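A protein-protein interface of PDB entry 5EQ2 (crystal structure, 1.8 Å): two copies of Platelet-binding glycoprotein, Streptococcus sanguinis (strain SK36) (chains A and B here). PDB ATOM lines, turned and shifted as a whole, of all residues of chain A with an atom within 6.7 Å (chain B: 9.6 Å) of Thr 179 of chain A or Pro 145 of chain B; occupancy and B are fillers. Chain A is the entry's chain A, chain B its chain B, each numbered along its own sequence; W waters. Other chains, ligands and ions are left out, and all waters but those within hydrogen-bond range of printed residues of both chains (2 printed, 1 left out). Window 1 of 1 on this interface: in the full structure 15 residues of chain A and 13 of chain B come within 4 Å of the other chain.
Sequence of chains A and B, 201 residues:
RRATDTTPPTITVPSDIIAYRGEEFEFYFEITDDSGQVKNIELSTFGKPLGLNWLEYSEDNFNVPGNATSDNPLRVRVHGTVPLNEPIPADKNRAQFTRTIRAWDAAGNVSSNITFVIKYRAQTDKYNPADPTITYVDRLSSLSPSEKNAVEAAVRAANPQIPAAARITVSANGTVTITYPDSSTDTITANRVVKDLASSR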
ATOM      1  N   LEU A  84     -29.050  20.493  12.386  1.00  0.00           N
ATOM      2  CA  LEU A  84     -28.437  19.256  11.930  1.00  0.00           C
ATOM      3  C   LEU A  84     -28.505  19.115  10.428  1.00  0.00           C
ATOM      4  O   LEU A  84     -27.588  18.568   9.811  1.00  0.00           O
ATOM      5  CB  LEU A  84     -29.141  18.053  12.555  1.00  0.00           C
ATOM      6  CG  LEU A  84     -28.622  17.360  13.799  1.00  0.00           C
ATOM      7  CD1 LEU A  84     -29.443  16.087  13.976  1.00  0.00           C
ATOM      8  CD2 LEU A  84     -27.167  17.035  13.670  1.00  0.00           C
ATOM      9  N   GLN A 123     -20.118  17.678  10.184  1.00  0.00           N
ATOM     10  CA  GLN A 123     -19.365  17.157  11.320  1.00  0.00           C
ATOM     11  C   GLN A 123     -18.175  16.332  10.873  1.00  0.00           C
ATOM     12  O   GLN A 123     -17.174  16.239  11.596  1.00  0.00           O
ATOM     13  CB  GLN A 123     -20.278  16.326  12.212  1.00  0.00           C
ATOM     14  CG  GLN A 123     -21.202  17.184  13.037  1.00  0.00           C
ATOM     15  CD  GLN A 123     -22.230  16.348  13.746  1.00  0.00           C
ATOM     16  OE1 GLN A 123     -23.046  15.690  13.108  1.00  0.00           O
ATOM     17  NE2 GLN A 123     -22.188  16.354  15.063  1.00  0.00           N
ATOM     18  N   ALA A 165     -23.469  10.088  19.711  1.00  0.00           N
ATOM     19  CA  ALA A 165     -24.620   9.946  18.833  1.00  0.00           C
ATOM     20  C   ALA A 165     -24.239   9.610  17.393  1.00  0.00           C
ATOM     21  O   ALA A 165     -25.135   9.400  16.575  1.00  0.00           O
ATOM     22  CB  ALA A 165     -25.477  11.215  18.854  1.00  0.00           C
ATOM     23  N   ALA A 166     -22.952   9.587  17.054  1.00  0.00           N
ATOM     24  CA  ALA A 166     -22.548   9.016  15.779  1.00  0.00           C
ATOM     25  C   ALA A 166     -22.804   7.509  15.797  1.00  0.00           C
ATOM     26  O   ALA A 166     -22.633   6.841  16.820  1.00  0.00           O
ATOM     27  CB  ALA A 166     -21.073   9.282  15.499  1.00  0.00           C
ATOM     28  N   ARG A 167     -23.190   6.969  14.645  1.00  0.00           N
ATOM     29  CA  ARG A 167     -23.502   5.548  14.532  1.00  0.00           C
ATOM     30  C   ARG A 167     -22.455   4.843  13.689  1.00  0.00           C
ATOM     31  O   ARG A 167     -22.132   5.295  12.586  1.00  0.00           O
ATOM     32  CB  ARG A 167     -24.891   5.334  13.932  1.00  0.00           C
ATOM     33  CG  ARG A 167     -25.282   3.831  13.874  1.00  0.00           C
ATOM     34  CD  ARG A 167     -26.781   3.646  13.863  1.00  0.00           C
ATOM     35  NE  ARG A 167     -27.176   2.218  13.888  1.00  0.00           N
ATOM     36  CZ  ARG A 167     -27.242   1.468  14.973  1.00  0.00           C
ATOM     37  NH1 ARG A 167     -26.928   1.966  16.169  1.00  0.00           N
ATOM     38  NH2 ARG A 167     -27.614   0.179  14.862  1.00  0.00           N
ATOM     39  N   ILE A 168     -21.929   3.736  14.215  1.00  0.00           N
ATOM     40  CA  ILE A 168     -20.850   2.987  13.594  1.00  0.00           C
ATOM     41  C   ILE A 168     -21.443   1.714  13.021  1.00  0.00           C
ATOM     42  O   ILE A 168     -22.009   0.907  13.763  1.00  0.00           O
ATOM     43  CB  ILE A 168     -19.734   2.661  14.595  1.00  0.00           C
ATOM     44  CG1 ILE A 168     -19.144   3.953  15.166  1.00  0.00           C
ATOM     45  CG2 ILE A 168     -18.658   1.885  13.900  1.00  0.00           C
ATOM     46  CD1 ILE A 168     -18.110   3.712  16.241  1.00  0.00           C
ATOM     47  N   THR A 169     -21.340   1.541  11.707  1.00  0.00           N
ATOM     48  CA  THR A 169     -21.805   0.318  11.055  1.00  0.00           C
ATOM     49  C   THR A 169     -20.633  -0.405  10.410  1.00  0.00           C
ATOM     50  O   THR A 169     -19.587   0.192  10.107  1.00  0.00           O
ATOM     51  CB  THR A 169     -22.882   0.597   9.978  1.00  0.00           C
ATOM     52  OG1 THR A 169     -22.425   1.629   9.096  1.00  0.00           O
ATOM     53  CG2 THR A 169     -24.195   1.030  10.604  1.00  0.00           C
ATOM     54  N   THR A 177     -18.290   2.205   8.454  1.00  0.00           N
ATOM     55  CA  THR A 177     -18.855   3.523   8.193  1.00  0.00           C
ATOM     56  C   THR A 177     -19.172   4.186   9.519  1.00  0.00           C
ATOM     57  O   THR A 177     -19.809   3.573  10.377  1.00  0.00           O
ATOM     58  CB  THR A 177     -20.129   3.438   7.346  1.00  0.00           C
ATOM     59  OG1 THR A 177     -19.848   2.799   6.094  1.00  0.00           O
ATOM     60  CG2 THR A 177     -20.683   4.857   7.074  1.00  0.00           C
ATOM     61  N   ILE A 178     -18.726   5.427   9.693  1.00  0.00           N
ATOM     62  CA  ILE A 178     -19.120   6.254  10.825  1.00  0.00           C
ATOM     63  C   ILE A 178     -20.061   7.317  10.284  1.00  0.00           C
ATOM     64  O   ILE A 178     -19.675   8.112   9.416  1.00  0.00           O
ATOM     65  CB  ILE A 178     -17.913   6.896  11.522  1.00  0.00           C
ATOM     66  CG1 ILE A 178     -16.932   5.821  11.994  1.00  0.00           C
ATOM     67  CG2 ILE A 178     -18.383   7.814  12.679  1.00  0.00           C
ATOM     68  CD1 ILE A 178     -15.595   6.365  12.407  1.00  0.00           C
ATOM     69  N   THR A 179     -21.300   7.308  10.759  1.00  0.00           N
ATOM     70  CA  THR A 179     -22.287   8.292  10.334  1.00  0.00           C
ATOM     71  C   THR A 179     -22.530   9.244  11.494  1.00  0.00           C
ATOM     72  O   THR A 179     -23.143   8.873  12.498  1.00  0.00           O
ATOM     73  CB  THR A 179     -23.572   7.625   9.871  1.00  0.00           C
ATOM     74  OG1 THR A 179     -23.267   6.723   8.794  1.00  0.00           O
ATOM     75  CG2 THR A 179     -24.563   8.681   9.402  1.00  0.00           C
ATOM     76  N   TYR A 180     -22.068  10.484  11.333  1.00  0.00           N
ATOM     77  CA  TYR A 180     -22.197  11.494  12.362  1.00  0.00           C
ATOM     78  C   TYR A 180     -23.646  11.946  12.504  1.00  0.00           C
ATOM     79  O   TYR A 180     -24.471  11.707  11.625  1.00  0.00           O
ATOM     80  CB  TYR A 180     -21.274  12.679  12.028  1.00  0.00           C
ATOM     81  CG  TYR A 180     -19.831  12.236  11.991  1.00  0.00           C
ATOM     82  CD1 TYR A 180     -19.136  12.002  13.164  1.00  0.00           C
ATOM     83  CD2 TYR A 180     -19.181  12.006  10.785  1.00  0.00           C
ATOM     84  CE1 TYR A 180     -17.824  11.574  13.141  1.00  0.00           C
ATOM     85  CE2 TYR A 180     -17.865  11.581  10.750  1.00  0.00           C
ATOM     86  CZ  TYR A 180     -17.195  11.369  11.935  1.00  0.00           C
ATOM     87  OH  TYR A 180     -15.886  10.934  11.923  1.00  0.00           O
ATOM     88  N   PRO A 181     -23.988  12.592  13.622  1.00  0.00           N
ATOM     89  CA  PRO A 181     -25.396  12.954  13.845  1.00  0.00           C
ATOM     90  C   PRO A 181     -26.026  13.751  12.728  1.00  0.00           C
ATOM     91  O   PRO A 181     -27.234  13.625  12.533  1.00  0.00           O
ATOM     92  CB  PRO A 181     -25.338  13.732  15.160  1.00  0.00           C
ATOM     93  CG  PRO A 181     -24.231  13.041  15.909  1.00  0.00           C
ATOM     94  CD  PRO A 181     -23.188  12.710  14.858  1.00  0.00           C
ATOM     95  N   ASP A 182     -25.256  14.541  11.963  1.00  0.00           N
ATOM     96  CA  ASP A 182     -25.780  15.295  10.828  1.00  0.00           C
ATOM     97  C   ASP A 182     -25.808  14.486   9.530  1.00  0.00           C
ATOM     98  O   ASP A 182     -26.068  15.054   8.465  1.00  0.00           O
ATOM     99  CB  ASP A 182     -24.974  16.598  10.626  1.00  0.00           C
ATOM    100  CG  ASP A 182     -23.585  16.368  10.027  1.00  0.00           C
ATOM    101  OD1 ASP A 182     -23.048  15.237  10.091  1.00  0.00           O
ATOM    102  OD2 ASP A 182     -23.002  17.337   9.490  1.00  0.00           O
ATOM    103  N   SER A 183     -25.549  13.176   9.598  1.00  0.00           N
ATOM    104  CA  SER A 183     -25.560  12.240   8.477  1.00  0.00           C
ATOM    105  C   SER A 183     -24.379  12.373   7.515  1.00  0.00           C
ATOM    106  O   SER A 183     -24.337  11.616   6.527  1.00  0.00           O
ATOM    107  CB  SER A 183     -26.863  12.302   7.669  1.00  0.00           C
ATOM    108  OG  SER A 183     -27.928  11.796   8.457  1.00  0.00           O
ATOM    109  N   SER A 184     -23.409  13.258   7.772  1.00  0.00           N
ATOM    110  CA  SER A 184     -22.122  13.174   7.075  1.00  0.00           C
ATOM    111  C   SER A 184     -21.356  11.955   7.596  1.00  0.00           C
ATOM    112  O   SER A 184     -21.701  11.378   8.633  1.00  0.00           O
ATOM    113  CB  SER A 184     -21.296  14.464   7.251  1.00  0.00           C
ATOM    114  OG  SER A 184     -20.856  14.645   8.590  1.00  0.00           O
ATOM    115  N   THR A 185     -20.342  11.518   6.849  1.00  0.00           N
ATOM    116  CA  THR A 185     -19.756  10.214   7.155  1.00  0.00           C
ATOM    117  C   THR A 185     -18.238  10.218   7.077  1.00  0.00           C
ATOM    118  O   THR A 185     -17.594  11.142   6.578  1.00  0.00           O
ATOM    119  CB  THR A 185     -20.247   9.093   6.222  1.00  0.00           C
ATOM    120  OG1 THR A 185     -19.804   9.339   4.878  1.00  0.00           O
ATOM    121  CG2 THR A 185     -21.748   8.952   6.249  1.00  0.00           C
ATOM    122  N   ASP A 186     -17.688   9.106   7.541  1.00  0.00           N
ATOM    123  CA  ASP A 186     -16.292   8.733   7.401  1.00  0.00           C
ATOM    124  C   ASP A 186     -16.260   7.226   7.199  1.00  0.00           C
ATOM    125  O   ASP A 186     -17.144   6.512   7.689  1.00  0.00           O
ATOM    126  CB  ASP A 186     -15.499   9.161   8.641  1.00  0.00           C
ATOM    127  CG  ASP A 186     -14.947  10.548   8.502  1.00  0.00           C
ATOM    128  OD1 ASP A 186     -14.698  11.218   9.521  1.00  0.00           O
ATOM    129  OD2 ASP A 186     -14.712  10.905   7.338  1.00  0.00           O
ATOM    130  N   THR B 135     -38.583   4.585  21.691  1.00  0.00           N
ATOM    131  CA  THR B 135     -37.776   5.729  21.277  1.00  0.00           C
ATOM    132  C   THR B 135     -38.640   6.656  20.426  1.00  0.00           C
ATOM    133  O   THR B 135     -39.280   6.204  19.470  1.00  0.00           O
ATOM    134  CB  THR B 135     -36.557   5.271  20.465  1.00  0.00           C
ATOM    135  OG1 THR B 135     -35.761   4.370  21.248  1.00  0.00           O
ATOM    136  CG2 THR B 135     -35.701   6.470  20.022  1.00  0.00           C
ATOM    137  N   VAL B 137     -39.029   9.595  17.672  1.00  0.00           N
ATOM    138  CA  VAL B 137     -38.234   9.969  16.511  1.00  0.00           C
ATOM    139  C   VAL B 137     -38.899  11.131  15.781  1.00  0.00           C
ATOM    140  O   VAL B 137     -40.102  11.369  15.907  1.00  0.00           O
ATOM    141  CB  VAL B 137     -38.012   8.786  15.537  1.00  0.00           C
ATOM    142  CG1 VAL B 137     -37.331   7.615  16.252  1.00  0.00           C
ATOM    143  CG2 VAL B 137     -39.324   8.332  14.945  1.00  0.00           C
ATOM    144  N   ARG B 139     -38.792  11.658  12.237  1.00  0.00           N
ATOM    145  CA  ARG B 139     -39.467  11.133  11.054  1.00  0.00           C
ATOM    146  C   ARG B 139     -39.493   9.613  11.128  1.00  0.00           C
ATOM    147  O   ARG B 139     -38.444   8.982  11.281  1.00  0.00           O
ATOM    148  CB  ARG B 139     -38.778  11.579   9.766  1.00  0.00           C
ATOM    149  CG  ARG B 139     -38.325  13.031   9.770  1.00  0.00           C
ATOM    150  CD  ARG B 139     -37.438  13.327   8.565  1.00  0.00           C
ATOM    151  NE  ARG B 139     -38.016  12.796   7.331  1.00  0.00           N
ATOM    152  CZ  ARG B 139     -37.350  12.655   6.189  1.00  0.00           C
ATOM    153  NH1 ARG B 139     -36.071  13.001   6.117  1.00  0.00           N
ATOM    154  NH2 ARG B 139     -37.962  12.159   5.120  1.00  0.00           N
ATOM    155  N   SER B 142     -37.509   7.792   8.289  1.00  0.00           N
ATOM    156  CA  SER B 142     -36.096   8.124   8.117  1.00  0.00           C
ATOM    157  C   SER B 142     -35.510   8.458   9.494  1.00  0.00           C
ATOM    158  O   SER B 142     -35.419   9.619   9.904  1.00  0.00           O
ATOM    159  CB  SER B 142     -35.913   9.283   7.139  1.00  0.00           C
ATOM    160  OG  SER B 142     -34.544   9.607   6.993  1.00  0.00           O
ATOM    161  N   LEU B 143     -35.092   7.417  10.215  1.00  0.00           N
ATOM    162  CA  LEU B 143     -34.456   7.629  11.508  1.00  0.00           C
ATOM    163  C   LEU B 143     -33.105   8.309  11.331  1.00  0.00           C
ATOM    164  O   LEU B 143     -32.411   8.099  10.333  1.00  0.00           O
ATOM    165  CB  LEU B 143     -34.268   6.301  12.245  1.00  0.00           C
ATOM    166  CG  LEU B 143     -35.374   5.894  13.227  1.00  0.00           C
ATOM    167  CD1 LEU B 143     -36.723   5.699  12.531  1.00  0.00           C
ATOM    168  CD2 LEU B 143     -34.965   4.630  13.988  1.00  0.00           C
ATOM    169  N   SER B 144     -32.735   9.127  12.316  1.00  0.00           N
ATOM    170  CA  SER B 144     -31.416   9.732  12.342  1.00  0.00           C
ATOM    171  C   SER B 144     -30.409   8.745  12.920  1.00  0.00           C
ATOM    172  O   SER B 144     -30.796   7.754  13.546  1.00  0.00           O
ATOM    173  CB  SER B 144     -31.438  11.010  13.176  1.00  0.00           C
ATOM    174  OG  SER B 144     -31.389  10.727  14.569  1.00  0.00           O
ATOM    175  N   PRO B 145     -29.108   8.975  12.710  1.00  0.00           N
ATOM    176  CA  PRO B 145     -28.114   8.114  13.373  1.00  0.00           C
ATOM    177  C   PRO B 145     -28.306   8.046  14.878  1.00  0.00           C
ATOM    178  O   PRO B 145     -28.198   6.965  15.469  1.00  0.00           O
ATOM    179  CB  PRO B 145     -26.777   8.770  13.005  1.00  0.00           C
ATOM    180  CG  PRO B 145     -27.051   9.546  11.762  1.00  0.00           C
ATOM    181  CD  PRO B 145     -28.487   9.952  11.790  1.00  0.00           C
ATOM    182  N   SER B 146     -28.609   9.182  15.514  1.00  0.00           N
ATOM    183  CA  SER B 146     -28.732   9.205  16.965  1.00  0.00           C
ATOM    184  C   SER B 146     -29.926   8.384  17.423  1.00  0.00           C
ATOM    185  O   SER B 146     -29.864   7.696  18.451  1.00  0.00           O
ATOM    186  CB  SER B 146     -28.858  10.649  17.455  1.00  0.00           C
ATOM    187  OG  SER B 146     -29.075  10.671  18.853  1.00  0.00           O
ATOM    188  N   GLU B 147     -31.019   8.447  16.665  1.00  0.00           N
ATOM    189  CA  GLU B 147     -32.213   7.681  16.987  1.00  0.00           C
ATOM    190  C   GLU B 147     -31.968   6.190  16.839  1.00  0.00           C
ATOM    191  O   GLU B 147     -32.433   5.403  17.665  1.00  0.00           O
ATOM    192  CB  GLU B 147     -33.362   8.119  16.088  1.00  0.00           C
ATOM    193  CG  GLU B 147     -33.890   9.506  16.478  1.00  0.00           C
ATOM    194  CD  GLU B 147     -34.653  10.187  15.362  1.00  0.00           C
ATOM    195  OE1 GLU B 147     -34.674   9.645  14.234  1.00  0.00           O
ATOM    196  OE2 GLU B 147     -35.214  11.282  15.618  1.00  0.00           O
ATOM    197  N   LYS B 148     -31.243   5.781  15.792  1.00  0.00           N
ATOM    198  CA  LYS B 148     -30.904   4.364  15.648  1.00  0.00           C
ATOM    199  C   LYS B 148     -30.054   3.879  16.813  1.00  0.00           C
ATOM    200  O   LYS B 148     -30.282   2.782  17.349  1.00  0.00           O
ATOM    201  CB  LYS B 148     -30.182   4.128  14.322  1.00  0.00           C
ATOM    202  CG  LYS B 148     -31.006   4.462  13.102  1.00  0.00           C
ATOM    203  CD  LYS B 148     -30.242   4.187  11.821  1.00  0.00           C
ATOM    204  CE  LYS B 148     -31.070   4.572  10.606  1.00  0.00           C
ATOM    205  NZ  LYS B 148     -30.276   4.527   9.343  1.00  0.00           N
ATOM    206  N   ASN B 149     -29.062   4.673  17.216  1.00  0.00           N
ATOM    207  CA  ASN B 149     -28.279   4.336  18.404  1.00  0.00           C
ATOM    208  C   ASN B 149     -29.185   4.112  19.611  1.00  0.00           C
ATOM    209  O   ASN B 149     -29.000   3.156  20.379  1.00  0.00           O
ATOM    210  CB  ASN B 149     -27.284   5.456  18.720  1.00  0.00           C
ATOM    211  CG  ASN B 149     -25.959   5.293  18.013  1.00  0.00           C
ATOM    212  OD1 ASN B 149     -25.820   4.470  17.115  1.00  0.00           O
ATOM    213  ND2 ASN B 149     -24.966   6.080  18.433  1.00  0.00           N
ATOM    214  N   ALA B 150     -30.163   5.007  19.800  1.00  0.00           N
ATOM    215  CA  ALA B 150     -31.055   4.914  20.952  1.00  0.00           C
ATOM    216  C   ALA B 150     -31.914   3.658  20.890  1.00  0.00           C
ATOM    217  O   ALA B 150     -32.083   2.959  21.904  1.00  0.00           O
ATOM    218  CB  ALA B 150     -31.941   6.156  21.032  1.00  0.00           C
ATOM    219  N   VAL B 151     -32.483   3.372  19.714  1.00  0.00           N
ATOM    220  CA  VAL B 151     -33.230   2.126  19.521  1.00  0.00           C
ATOM    221  C   VAL B 151     -32.377   0.920  19.898  1.00  0.00           C
ATOM    222  O   VAL B 151     -32.808   0.039  20.656  1.00  0.00           O
ATOM    223  CB  VAL B 151     -33.718   2.013  18.067  1.00  0.00           C
ATOM    224  CG1 VAL B 151     -34.168   0.552  17.788  1.00  0.00           C
ATOM    225  CG2 VAL B 151     -34.835   2.981  17.789  1.00  0.00           C
ATOM    226  N   GLU B 152     -31.156   0.846  19.354  1.00  0.00           N
ATOM    227  CA  GLU B 152     -30.334  -0.331  19.620  1.00  0.00           C
ATOM    228  C   GLU B 152     -30.056  -0.468  21.110  1.00  0.00           C
ATOM    229  O   GLU B 152     -30.199  -1.560  21.675  1.00  0.00           O
ATOM    230  CB  GLU B 152     -29.013  -0.284  18.826  1.00  0.00           C
ATOM    231  CG  GLU B 152     -28.106  -1.493  19.150  1.00  0.00           C
ATOM    232  CD  GLU B 152     -26.755  -1.490  18.426  1.00  0.00           C
ATOM    233  OE1 GLU B 152     -26.515  -0.602  17.569  1.00  0.00           O
ATOM    234  OE2 GLU B 152     -25.922  -2.390  18.717  1.00  0.00           O
ATOM    235  N   ALA B 153     -29.697   0.639  21.775  1.00  0.00           N
ATOM    236  CA  ALA B 153     -29.402   0.588  23.205  1.00  0.00           C
ATOM    237  C   ALA B 153     -30.606   0.102  23.997  1.00  0.00           C
ATOM    238  O   ALA B 153     -30.461  -0.609  25.003  1.00  0.00           O
ATOM    239  CB  ALA B 153     -28.989   1.969  23.709  1.00  0.00           C
ATOM    240  N   VAL B 170     -30.664  -1.664  12.948  1.00  0.00           N
ATOM    241  CA  VAL B 170     -31.870  -0.838  12.927  1.00  0.00           C
ATOM    242  C   VAL B 170     -31.987  -0.243  11.531  1.00  0.00           C
ATOM    243  O   VAL B 170     -31.049   0.399  11.050  1.00  0.00           O
ATOM    244  CB  VAL B 170     -31.822   0.279  13.983  1.00  0.00           C
ATOM    245  CG1 VAL B 170     -33.168   0.996  14.040  1.00  0.00           C
ATOM    246  CG2 VAL B 170     -31.447  -0.280  15.368  1.00  0.00           C
ATOM    247  N   SER B 171     -33.123  -0.460  10.875  1.00  0.00           N
ATOM    248  CA  SER B 171     -33.266   0.049   9.520  1.00  0.00           C
ATOM    249  C   SER B 171     -33.725   1.514   9.548  1.00  0.00           C
ATOM    250  O   SER B 171     -33.950   2.109  10.601  1.00  0.00           O
ATOM    251  CB  SER B 171     -34.264  -0.784   8.727  1.00  0.00           C
ATOM    252  OG  SER B 171     -35.575  -0.546   9.202  1.00  0.00           O
ATOM    253  N   ALA B 172     -33.899   2.083   8.356  1.00  0.00           N
ATOM    254  CA  ALA B 172     -34.330   3.474   8.248  1.00  0.00           C
ATOM    255  C   ALA B 172     -35.669   3.731   8.931  1.00  0.00           C
ATOM    256  O   ALA B 172     -35.914   4.848   9.408  1.00  0.00           O
ATOM    257  CB  ALA B 172     -34.414   3.883   6.777  1.00  0.00           C
HETATM  258  O   HOH W   1     -28.614  12.211  14.671  1.00  0.00           O
HETATM  259  O   HOH W   2     -22.802   3.053  16.934  1.00  0.00           O
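Water W1 lies within hydrogen-bond range of the backbone carbonyl oxygen (O) of Pro 181 of chain A (2.9 Å), the backbone NH (N) of Ser 146 of chain B (3.1 Å) and the side-chain hydroxyl (OG) of Ser 144 of chain B (3.1 Å).
Water W2 lies within hydrogen-bond range of N of Ile 168 of chain A (2.9 Å) and OD1 of Asn 149 of chain B (3.3 Å).
OD1 of Asn 149 of chain B is in hydrogen-bond range of NH1 of Arg 167 of chain A, 2.9 Å away.
The backbone carbonyl oxygen of Ala 166 of chain A is in hydrogen-bond range of the side-chain amide nitrogen of Asn 149 of chain B.
The side-chain carboxylate of Glu 152 of chain B lies close to the guanidinium group of Arg 167 of chain A (3.0 Å).
Of chain B, only Pro 145 (3.5 Å) comes within 4 Å of Thr 179 of chain A.
Pro 145 of chain B touches just these residues of chain A: Ala 165 (3.8 Å), Arg 167 (3.95 Å), Thr 179 (3.5 Å), Tyr 180 (3.4 Å), Pro 181 (3.95 Å) and Ser 183 (3.8 Å).
Ala 166 of chain A touches one residue of chain B.
Of chain B, only Pro 145 (3.8 Å) comes within 4 Å of Ser 183 of chain A.
Printed residues of chain A within 4 Å of Glu 152 of chain B: Arg 167 (3.0 Å).
Printed residues of chain A within 4 Å of Asn 149 of chain B: Ala 165 (3.8 Å), Ala 166 (2.9 Å) and Arg 167 (2.9 Å).
Of the printed residues of chain A, Ser 146 of chain B touches Ala 165 (3.6 Å).
Ile 168 of chain A touches none of the printed residues of chain B.
Ser 171 of chain B touches none of the printed residues of chain A.
The nearest residue of chain A that does not touch Pro 145 of chain B is Ala 166 of chain A (5.0 Å).
No position is printed for both chains.
Of the 13 pairs that touch across the chains among the printed residues, none has its exchanged pair printed and touching as well.
Of the 18 printed residues of chain B, 6 touch a printed residue of chain A.
Hydrophobic or aromatic side chains of chain B within 4 Å of the printed part of chain A: Pro 145 and Val 170.
Among the printed residues, 13 pairs touch across the chains.
Among the printed residues, Asp or Glu carboxylates within 4 Å of a Lys or Arg side-chain nitrogen of the other chain: Arg 167 of chain A with Glu 152 of chain B.
Among the printed residues, merely in contact across the chains: Tyr 180 of chain A with Pro 145 of chain B (3.4 Å), Arg 167 of chain A with Lys 148 of chain B (3.5 Å), Thr 179 of chain A with Pro 145 of chain B (3.5 Å), Ala 165 of chain A with Ser 146 of chain B (3.6 Å), Ala 165 of chain A with Asn 149 of chain B (3.8 Å), Ala 165 of chain A with Pro 145 of chain B (3.8 Å), Ser 183 of chain A with Pro 145 of chain B (3.8 Å), Arg 167 of chain A with Val 170 of chain B (3.9 Å), Arg 167 of chain A with Pro 145 of chain B (3.95 Å) and Pro 181 of chain A with Pro 145 of chain B (3.95 Å).
The backbone NH (N) of Thr 179 of chain A sits at hydrogen-bond distance from the backbone carbonyl oxygen (O) of Arg 167 of chain A (2.8 Å).
The side-chain hydroxyl (OH) of Tyr 180 of chain A sits close to the side-chain carboxylate (OD1) of Asp 186 of chain A, at 2.7 Å.
N of Ser 146 of chain B sits close to OG of Ser 144 of chain B (3.3 Å).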
